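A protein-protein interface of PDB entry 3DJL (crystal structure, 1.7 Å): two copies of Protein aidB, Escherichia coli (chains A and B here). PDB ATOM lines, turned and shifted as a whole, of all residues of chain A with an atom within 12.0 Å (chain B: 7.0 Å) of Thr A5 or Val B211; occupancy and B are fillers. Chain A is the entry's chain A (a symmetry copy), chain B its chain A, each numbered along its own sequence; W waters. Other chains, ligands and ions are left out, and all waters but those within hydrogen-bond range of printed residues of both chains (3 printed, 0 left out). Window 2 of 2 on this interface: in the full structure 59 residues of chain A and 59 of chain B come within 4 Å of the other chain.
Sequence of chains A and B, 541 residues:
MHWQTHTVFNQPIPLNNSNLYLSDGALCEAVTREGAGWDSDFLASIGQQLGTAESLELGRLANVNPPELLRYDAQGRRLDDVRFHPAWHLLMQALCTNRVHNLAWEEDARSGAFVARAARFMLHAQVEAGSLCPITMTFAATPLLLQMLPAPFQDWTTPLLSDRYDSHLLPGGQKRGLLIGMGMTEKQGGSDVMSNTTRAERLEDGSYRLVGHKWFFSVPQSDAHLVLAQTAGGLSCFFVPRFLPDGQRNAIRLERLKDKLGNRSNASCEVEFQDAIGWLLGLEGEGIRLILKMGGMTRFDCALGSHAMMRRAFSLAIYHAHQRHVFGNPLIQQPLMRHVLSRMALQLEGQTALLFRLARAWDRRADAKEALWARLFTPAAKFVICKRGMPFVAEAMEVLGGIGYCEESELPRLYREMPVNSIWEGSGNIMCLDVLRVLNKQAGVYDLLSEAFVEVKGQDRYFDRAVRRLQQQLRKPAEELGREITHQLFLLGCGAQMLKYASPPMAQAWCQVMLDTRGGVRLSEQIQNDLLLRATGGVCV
The backbone carbonyl oxygen (O) of Gly B212 lies within hydrogen-bond range of the side-chain hydroxyl (OG1) of Thr A5 (3.3 Å).
The side-chain carboxylate of Glu B272 sits at hydrogen-bond distance from the side-chain hydroxyl of Thr A5 (2.9 Å).
N of Arg B253 is in hydrogen-bond range of O of Glu B272, at 2.8 Å.
The side-chain carboxylate of Glu B186 is in hydrogen-bond range of the backbone NH of Thr B197 (2.8 Å).
A ring nitrogen (ND1) of His A6 lies within hydrogen-bond range of the side-chain hydroxyl (OG1) of Thr A5.
O of His B213 sits at hydrogen-bond distance from OG1 of Thr B198 (3.0 Å).
The backbone NH (N) of Phe B273 sits at hydrogen-bond distance from the backbone carbonyl oxygen (O) of Gly B212, at 2.9 Å.
The backbone carbonyl oxygen of Val B211 lies within hydrogen-bond range of the backbone NH of Arg B199 (2.9 Å).
Thr A5 touches Val B211 (O to CG1, 3.7 Å).
Thr A5 touches Phe B273.
His A6 touches His B213 (CG to CD2, 3.5 Å).
His A6 touches Glu B272.
CE2 of Phe A9 touches CG2 of Thr B197 (3.9 Å).
No residue of chain A comes within 4 Å of Thr B198.
No residue of chain A comes within 4 Å of Ala B200.
No residue of chain A comes within 4 Å of Arg B209.
No residue of chain A comes within 4 Å of Leu B210.
Printed residues of chain A within 4 Å of Gly B212: Thr A5 (3.3 Å).
Of the printed residues of chain A, Glu B272 touches Thr A5 (2.9 Å) and His A6 (3.5 Å).
Phe B273 touches just one residue of chain A: Thr A5.
No residue of chain A comes within 4 Å of Asp B275.
No residue of chain A comes within 4 Å of Ala B276.
Printed residues of chain B within 4 Å of His A6: His B213 (3.5 Å) and Glu B272 (3.5 Å).
Printed residues of chain A within 4 Å of Thr B197: Phe A9.
Arg B253 touches none of the printed residues of chain A.
The nearest residue of chain A that does not touch Val B211 is Gln A4 (5.1 Å).
The nearest printed residue of chain A that does not touch Thr B197 is His A6 (4.8 Å).
Hydrophobic or aromatic side chains of chain A within 4 Å of the printed part of chain B: His A6 and Phe A9.
Along chain A the printed residues that touch a printed residue of chain B span positions 5 to 9.
Hydrophobic or aromatic side chains of chain B that line the printed part of chain A: Val B211 and His B213.
Among the printed residues, 7 pairs touch across the chains.
Among the printed residues, no Asp or Glu carboxylate lies within 4 Å of a Lys or Arg side-chain nitrogen of the other chain.
No position is printed for both chains.
Of the 7 pairs that touch across the chains among the printed residues, none has its exchanged pair printed and touching as well.
Water W3 lies within hydrogen-bond range of OE1 of Glu B272 and N of Thr A5.
Water W1 bridges OG1 of Thr B197 and N of Thr A7.
Water W2 bridges the backbone carbonyl oxygen of Thr A5 (2.8 Å) and the backbone carbonyl oxygen of Thr B197 (3.4 Å).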
ATOM      1  N   TRP A   3      22.360  -0.027   6.254  1.00  0.00           N
ATOM      2  CA  TRP A   3      22.013   1.172   7.045  1.00  0.00           C
ATOM      3  C   TRP A   3      22.139   2.479   6.229  1.00  0.00           C
ATOM      4  O   TRP A   3      21.675   3.513   6.676  1.00  0.00           O
ATOM      5  CB  TRP A   3      22.919   1.250   8.274  1.00  0.00           C
ATOM      6  CG  TRP A   3      22.832   0.005   9.160  1.00  0.00           C
ATOM      7  CD1 TRP A   3      23.737  -1.011   9.240  1.00  0.00           C
ATOM      8  CD2 TRP A   3      21.794  -0.304  10.083  1.00  0.00           C
ATOM      9  NE1 TRP A   3      23.330  -1.936  10.172  1.00  0.00           N
ATOM     10  CE2 TRP A   3      22.137  -1.528  10.706  1.00  0.00           C
ATOM     11  CE3 TRP A   3      20.596   0.326  10.436  1.00  0.00           C
ATOM     12  CZ2 TRP A   3      21.322  -2.138  11.646  1.00  0.00           C
ATOM     13  CZ3 TRP A   3      19.782  -0.272  11.363  1.00  0.00           C
ATOM     14  CH2 TRP A   3      20.154  -1.492  11.983  1.00  0.00           C
ATOM     15  N   GLN A   4      22.756   2.429   5.056  1.00  0.00           N
ATOM     16  CA  GLN A   4      22.992   3.648   4.280  1.00  0.00           C
ATOM     17  C   GLN A   4      21.948   3.831   3.178  1.00  0.00           C
ATOM     18  O   GLN A   4      21.449   2.857   2.651  1.00  0.00           O
ATOM     19  CB  GLN A   4      24.368   3.599   3.619  1.00  0.00           C
ATOM     20  N   THR A   5      21.684   5.077   2.782  1.00  0.00           N
ATOM     21  CA  THR A   5      20.740   5.349   1.646  1.00  0.00           C
ATOM     22  C   THR A   5      21.477   5.670   0.332  1.00  0.00           C
ATOM     23  O   THR A   5      20.876   5.704  -0.757  1.00  0.00           O
ATOM     24  CB  THR A   5      19.847   6.549   1.994  1.00  0.00           C
ATOM     25  OG1 THR A   5      20.688   7.668   2.298  1.00  0.00           O
ATOM     26  CG2 THR A   5      18.994   6.250   3.236  1.00  0.00           C
ATOM     27  N   HIS A   6      22.784   5.891   0.435  1.00  0.00           N
ATOM     28  CA  HIS A   6      23.585   6.361  -0.679  1.00  0.00           C
ATOM     29  C   HIS A   6      25.073   6.213  -0.341  1.00  0.00           C
ATOM     30  O   HIS A   6      25.450   6.038   0.831  1.00  0.00           O
ATOM     31  CB  HIS A   6      23.241   7.864  -0.988  1.00  0.00           C
ATOM     32  CG  HIS A   6      23.657   8.827   0.097  1.00  0.00           C
ATOM     33  ND1 HIS A   6      22.970   8.972   1.288  1.00  0.00           N
ATOM     34  CD2 HIS A   6      24.687   9.709   0.146  1.00  0.00           C
ATOM     35  CE1 HIS A   6      23.577   9.890   2.030  1.00  0.00           C
ATOM     36  NE2 HIS A   6      24.629  10.342   1.364  1.00  0.00           N
ATOM     37  N   THR A   7      25.906   6.318  -1.378  1.00  0.00           N
ATOM     38  CA  THR A   7      27.346   6.424  -1.256  1.00  0.00           C
ATOM     39  C   THR A   7      27.766   7.847  -1.578  1.00  0.00           C
ATOM     40  O   THR A   7      27.216   8.472  -2.500  1.00  0.00           O
ATOM     41  CB  THR A   7      28.005   5.473  -2.287  1.00  0.00           C
ATOM     42  OG1 THR A   7      27.679   4.128  -1.918  1.00  0.00           O
ATOM     43  CG2 THR A   7      29.526   5.638  -2.288  1.00  0.00           C
ATOM     44  N   VAL A   8      28.725   8.367  -0.832  1.00  0.00           N
ATOM     45  CA  VAL A   8      29.226   9.730  -1.101  1.00  0.00           C
ATOM     46  C   VAL A   8      30.380   9.622  -2.104  1.00  0.00           C
ATOM     47  O   VAL A   8      31.306   8.831  -1.919  1.00  0.00           O
ATOM     48  CB  VAL A   8      29.708  10.430   0.205  1.00  0.00           C
ATOM     49  CG1 VAL A   8      30.214  11.884  -0.075  1.00  0.00           C
ATOM     50  CG2 VAL A   8      28.629  10.430   1.237  1.00  0.00           C
ATOM     51  N   PHE A   9      30.326  10.391  -3.195  1.00  0.00           N
ATOM     52  CA  PHE A   9      31.398  10.379  -4.176  1.00  0.00           C
ATOM     53  C   PHE A   9      31.478  11.713  -4.900  1.00  0.00           C
ATOM     54  O   PHE A   9      30.563  12.535  -4.782  1.00  0.00           O
ATOM     55  CB  PHE A   9      31.287   9.222  -5.180  1.00  0.00           C
ATOM     56  CG  PHE A   9      30.097   9.308  -6.099  1.00  0.00           C
ATOM     57  CD1 PHE A   9      30.242   9.808  -7.402  1.00  0.00           C
ATOM     58  CD2 PHE A   9      28.813   8.956  -5.639  1.00  0.00           C
ATOM     59  CE1 PHE A   9      29.101   9.858  -8.264  1.00  0.00           C
ATOM     60  CE2 PHE A   9      27.679   9.046  -6.478  1.00  0.00           C
ATOM     61  CZ  PHE A   9      27.835   9.479  -7.787  1.00  0.00           C
ATOM     62  N   GLU B 186      22.488  16.744  -5.356  1.00  0.00           N
ATOM     63  CA  GLU B 186      23.071  15.679  -4.569  1.00  0.00           C
ATOM     64  C   GLU B 186      24.540  15.982  -4.324  1.00  0.00           C
ATOM     65  O   GLU B 186      25.092  16.913  -4.898  1.00  0.00           O
ATOM     66  CB  GLU B 186      22.871  14.298  -5.249  1.00  0.00           C
ATOM     67  CG  GLU B 186      21.367  13.917  -5.185  1.00  0.00           C
ATOM     68  CD  GLU B 186      21.048  12.521  -5.651  1.00  0.00           C
ATOM     69  OE1 GLU B 186      21.942  11.627  -5.691  1.00  0.00           O
ATOM     70  OE2 GLU B 186      19.850  12.310  -5.973  1.00  0.00           O
ATOM     71  N   THR B 197      21.915   9.882  -7.880  1.00  0.00           N
ATOM     72  CA  THR B 197      21.777   8.443  -7.586  1.00  0.00           C
ATOM     73  C   THR B 197      20.563   8.061  -6.749  1.00  0.00           C
ATOM     74  O   THR B 197      20.326   6.872  -6.508  1.00  0.00           O
ATOM     75  CB  THR B 197      23.010   7.875  -6.887  1.00  0.00           C
ATOM     76  OG1 THR B 197      23.288   8.685  -5.735  1.00  0.00           O
ATOM     77  CG2 THR B 197      24.215   7.912  -7.843  1.00  0.00           C
ATOM     78  N   THR B 198      19.753   9.037  -6.347  1.00  0.00           N
ATOM     79  CA  THR B 198      18.502   8.717  -5.661  1.00  0.00           C
ATOM     80  C   THR B 198      17.684   7.866  -6.607  1.00  0.00           C
ATOM     81  O   THR B 198      17.605   8.193  -7.817  1.00  0.00           O
ATOM     82  CB  THR B 198      17.736  10.017  -5.298  1.00  0.00           C
ATOM     83  OG1 THR B 198      18.517  10.718  -4.306  1.00  0.00           O
ATOM     84  CG2 THR B 198      16.361   9.694  -4.708  1.00  0.00           C
ATOM     85  N   ARG B 199      17.128   6.764  -6.071  1.00  0.00           N
ATOM     86  CA  ARG B 199      16.520   5.731  -6.899  1.00  0.00           C
ATOM     87  C   ARG B 199      15.066   5.577  -6.530  1.00  0.00           C
ATOM     88  O   ARG B 199      14.752   5.477  -5.342  1.00  0.00           O
ATOM     89  CB  ARG B 199      17.249   4.382  -6.674  1.00  0.00           C
ATOM     90  CG  ARG B 199      16.742   3.238  -7.526  1.00  0.00           C
ATOM     91  CD  ARG B 199      17.358   3.303  -8.919  1.00  0.00           C
ATOM     92  NE  ARG B 199      16.763   2.330  -9.829  1.00  0.00           N
ATOM     93  CZ  ARG B 199      16.922   2.361 -11.146  1.00  0.00           C
ATOM     94  NH1 ARG B 199      16.351   1.431 -11.906  1.00  0.00           N
ATOM     95  NH2 ARG B 199      17.647   3.322 -11.699  1.00  0.00           N
ATOM     96  N   ALA B 200      14.213   5.454  -7.547  1.00  0.00           N
ATOM     97  CA  ALA B 200      12.778   5.274  -7.375  1.00  0.00           C
ATOM     98  C   ALA B 200      12.328   3.948  -8.020  1.00  0.00           C
ATOM     99  O   ALA B 200      12.648   3.707  -9.187  1.00  0.00           O
ATOM    100  CB  ALA B 200      12.077   6.437  -8.045  1.00  0.00           C
ATOM    101  N   GLU B 201      11.666   3.095  -7.236  1.00  0.00           N
ATOM    102  CA  GLU B 201      11.119   1.805  -7.697  1.00  0.00           C
ATOM    103  C   GLU B 201       9.591   1.832  -7.692  1.00  0.00           C
ATOM    104  O   GLU B 201       8.968   2.203  -6.689  1.00  0.00           O
ATOM    105  CB  GLU B 201      11.604   0.683  -6.763  1.00  0.00           C
ATOM    106  N   ARG B 209       8.704   4.025  -4.524  1.00  0.00           N
ATOM    107  CA  ARG B 209       9.481   4.074  -3.296  1.00  0.00           C
ATOM    108  C   ARG B 209      10.884   4.649  -3.630  1.00  0.00           C
ATOM    109  O   ARG B 209      11.548   4.152  -4.545  1.00  0.00           O
ATOM    110  CB  ARG B 209       9.551   2.624  -2.801  1.00  0.00           C
ATOM    111  CG  ARG B 209      10.609   2.225  -1.855  1.00  0.00           C
ATOM    112  CD  ARG B 209      10.414   0.705  -1.509  1.00  0.00           C
ATOM    113  NE  ARG B 209      10.930  -0.191  -2.544  1.00  0.00           N
ATOM    114  N   LEU B 210      11.294   5.700  -2.924  1.00  0.00           N
ATOM    115  CA  LEU B 210      12.589   6.389  -3.154  1.00  0.00           C
ATOM    116  C   LEU B 210      13.572   6.105  -2.038  1.00  0.00           C
ATOM    117  O   LEU B 210      13.217   6.165  -0.868  1.00  0.00           O
ATOM    118  CB  LEU B 210      12.405   7.915  -3.282  1.00  0.00           C
ATOM    119  CG  LEU B 210      11.884   8.460  -4.647  1.00  0.00           C
ATOM    120  CD1 LEU B 210      10.497   7.883  -5.017  1.00  0.00           C
ATOM    121  CD2 LEU B 210      11.797   9.980  -4.617  1.00  0.00           C
ATOM    122  N   VAL B 211      14.817   5.809  -2.420  1.00  0.00           N
ATOM    123  CA  VAL B 211      15.935   5.680  -1.466  1.00  0.00           C
ATOM    124  C   VAL B 211      17.067   6.536  -2.020  1.00  0.00           C
ATOM    125  O   VAL B 211      17.415   6.417  -3.207  1.00  0.00           O
ATOM    126  CB  VAL B 211      16.408   4.212  -1.332  1.00  0.00           C
ATOM    127  CG1 VAL B 211      17.567   4.147  -0.372  1.00  0.00           C
ATOM    128  CG2 VAL B 211      15.260   3.354  -0.813  1.00  0.00           C
ATOM    129  N   GLY B 212      17.569   7.460  -1.210  1.00  0.00           N
ATOM    130  CA  GLY B 212      18.699   8.293  -1.655  1.00  0.00           C
ATOM    131  C   GLY B 212      18.852   9.494  -0.744  1.00  0.00           C
ATOM    132  O   GLY B 212      18.570   9.413   0.460  1.00  0.00           O
ATOM    133  N   HIS B 213      19.308  10.607  -1.298  1.00  0.00           N
ATOM    134  CA  HIS B 213      19.587  11.801  -0.447  1.00  0.00           C
ATOM    135  C   HIS B 213      19.420  13.033  -1.305  1.00  0.00           C
ATOM    136  O   HIS B 213      19.442  12.943  -2.533  1.00  0.00           O
ATOM    137  CB  HIS B 213      20.997  11.782   0.139  1.00  0.00           C
ATOM    138  CG  HIS B 213      22.054  12.084  -0.884  1.00  0.00           C
ATOM    139  ND1 HIS B 213      22.769  13.268  -0.924  1.00  0.00           N
ATOM    140  CD2 HIS B 213      22.477  11.357  -1.942  1.00  0.00           C
ATOM    141  CE1 HIS B 213      23.612  13.239  -1.953  1.00  0.00           C
ATOM    142  NE2 HIS B 213      23.462  12.089  -2.569  1.00  0.00           N
ATOM    143  N   ALA B 229      14.700  11.778  -9.277  1.00  0.00           N
ATOM    144  CA  ALA B 229      15.236  10.444  -8.935  1.00  0.00           C
ATOM    145  C   ALA B 229      15.358   9.571 -10.172  1.00  0.00           C
ATOM    146  O   ALA B 229      14.624   9.760 -11.139  1.00  0.00           O
ATOM    147  CB  ALA B 229      14.363   9.764  -7.928  1.00  0.00           C
ATOM    148  N   ARG B 253      14.145  11.976   6.115  1.00  0.00           N
ATOM    149  CA  ARG B 253      14.907  12.183   7.339  1.00  0.00           C
ATOM    150  C   ARG B 253      15.733  13.434   7.194  1.00  0.00           C
ATOM    151  O   ARG B 253      16.546  13.554   6.268  1.00  0.00           O
ATOM    152  CB  ARG B 253      15.859  11.006   7.616  1.00  0.00           C
ATOM    153  CG  ARG B 253      15.176   9.695   7.683  1.00  0.00           C
ATOM    154  CD  ARG B 253      14.598   9.487   9.052  1.00  0.00           C
ATOM    155  NE  ARG B 253      13.207   9.918   9.124  1.00  0.00           N
ATOM    156  CZ  ARG B 253      12.171   9.176   8.735  1.00  0.00           C
ATOM    157  NH1 ARG B 253      12.365   7.967   8.201  1.00  0.00           N
ATOM    158  NH2 ARG B 253      10.944   9.659   8.842  1.00  0.00           N
ATOM    159  N   VAL B 271      19.125  15.948   3.529  1.00  0.00           N
ATOM    160  CA  VAL B 271      18.082  14.978   3.839  1.00  0.00           C
ATOM    161  C   VAL B 271      18.364  13.598   3.219  1.00  0.00           C
ATOM    162  O   VAL B 271      19.161  13.481   2.261  1.00  0.00           O
ATOM    163  CB  VAL B 271      16.683  15.439   3.363  1.00  0.00           C
ATOM    164  CG1 VAL B 271      16.400  16.855   3.866  1.00  0.00           C
ATOM    165  CG2 VAL B 271      16.593  15.368   1.829  1.00  0.00           C
ATOM    166  N   GLU B 272      17.699  12.566   3.743  1.00  0.00           N
ATOM    167  CA  GLU B 272      17.814  11.192   3.205  1.00  0.00           C
ATOM    168  C   GLU B 272      16.419  10.622   3.095  1.00  0.00           C
ATOM    169  O   GLU B 272      15.526  10.952   3.911  1.00  0.00           O
ATOM    170  CB  GLU B 272      18.733  10.295   4.073  1.00  0.00           C
ATOM    171  CG  GLU B 272      20.160  10.921   4.185  1.00  0.00           C
ATOM    172  CD  GLU B 272      21.215  10.034   4.822  1.00  0.00           C
ATOM    173  OE1 GLU B 272      20.953   8.828   4.996  1.00  0.00           O
ATOM    174  OE2 GLU B 272      22.325  10.575   5.173  1.00  0.00           O
ATOM    175  N   PHE B 273      16.209   9.845   2.029  1.00  0.00           N
ATOM    176  CA  PHE B 273      14.922   9.177   1.785  1.00  0.00           C
ATOM    177  C   PHE B 273      15.100   7.705   2.145  1.00  0.00           C
ATOM    178  O   PHE B 273      15.958   6.984   1.582  1.00  0.00           O
ATOM    179  CB  PHE B 273      14.522   9.286   0.317  1.00  0.00           C
ATOM    180  CG  PHE B 273      14.471  10.699  -0.189  1.00  0.00           C
ATOM    181  CD1 PHE B 273      13.521  11.598   0.289  1.00  0.00           C
ATOM    182  CD2 PHE B 273      15.368  11.115  -1.141  1.00  0.00           C
ATOM    183  CE1 PHE B 273      13.487  12.917  -0.180  1.00  0.00           C
ATOM    184  CE2 PHE B 273      15.354  12.427  -1.620  1.00  0.00           C
ATOM    185  CZ  PHE B 273      14.421  13.333  -1.121  1.00  0.00           C
ATOM    186  N   GLN B 274      14.272   7.274   3.094  1.00  0.00           N
ATOM    187  CA  GLN B 274      14.256   5.902   3.578  1.00  0.00           C
ATOM    188  C   GLN B 274      12.987   5.191   3.121  1.00  0.00           C
ATOM    189  O   GLN B 274      12.078   4.987   3.913  1.00  0.00           O
ATOM    190  CB  GLN B 274      14.389   5.894   5.112  1.00  0.00           C
ATOM    191  CG  GLN B 274      15.731   6.448   5.557  1.00  0.00           C
ATOM    192  CD  GLN B 274      16.004   6.269   7.052  1.00  0.00           C
ATOM    193  OE1 GLN B 274      17.150   6.120   7.465  1.00  0.00           O
ATOM    194  NE2 GLN B 274      14.970   6.280   7.848  1.00  0.00           N
ATOM    195  N   ASP B 275      12.942   4.807   1.848  1.00  0.00           N
ATOM    196  CA  ASP B 275      11.706   4.316   1.215  1.00  0.00           C
ATOM    197  C   ASP B 275      10.576   5.340   1.341  1.00  0.00           C
ATOM    198  O   ASP B 275       9.438   5.015   1.731  1.00  0.00           O
ATOM    199  CB  ASP B 275      11.274   2.982   1.785  1.00  0.00           C
ATOM    200  CG  ASP B 275      12.335   1.919   1.615  1.00  0.00           C
ATOM    201  OD1 ASP B 275      12.928   1.870   0.525  1.00  0.00           O
ATOM    202  OD2 ASP B 275      12.581   1.153   2.574  1.00  0.00           O
ATOM    203  N   ALA B 276      10.908   6.581   1.031  1.00  0.00           N
ATOM    204  CA  ALA B 276       9.866   7.620   0.950  1.00  0.00           C
ATOM    205  C   ALA B 276       8.979   7.294  -0.280  1.00  0.00           C
ATOM    206  O   ALA B 276       9.481   6.714  -1.270  1.00  0.00           O
ATOM    207  CB  ALA B 276      10.479   8.925   0.745  1.00  0.00           C
HETATM  208  O   HOH W   1      24.832   7.007  -4.232  1.00  0.00           O
HETATM  209  O   HOH W   2      21.444   6.275  -3.397  1.00  0.00           O
HETATM  210  O   HOH W   3      22.879   7.047   4.496  1.00  0.00           O
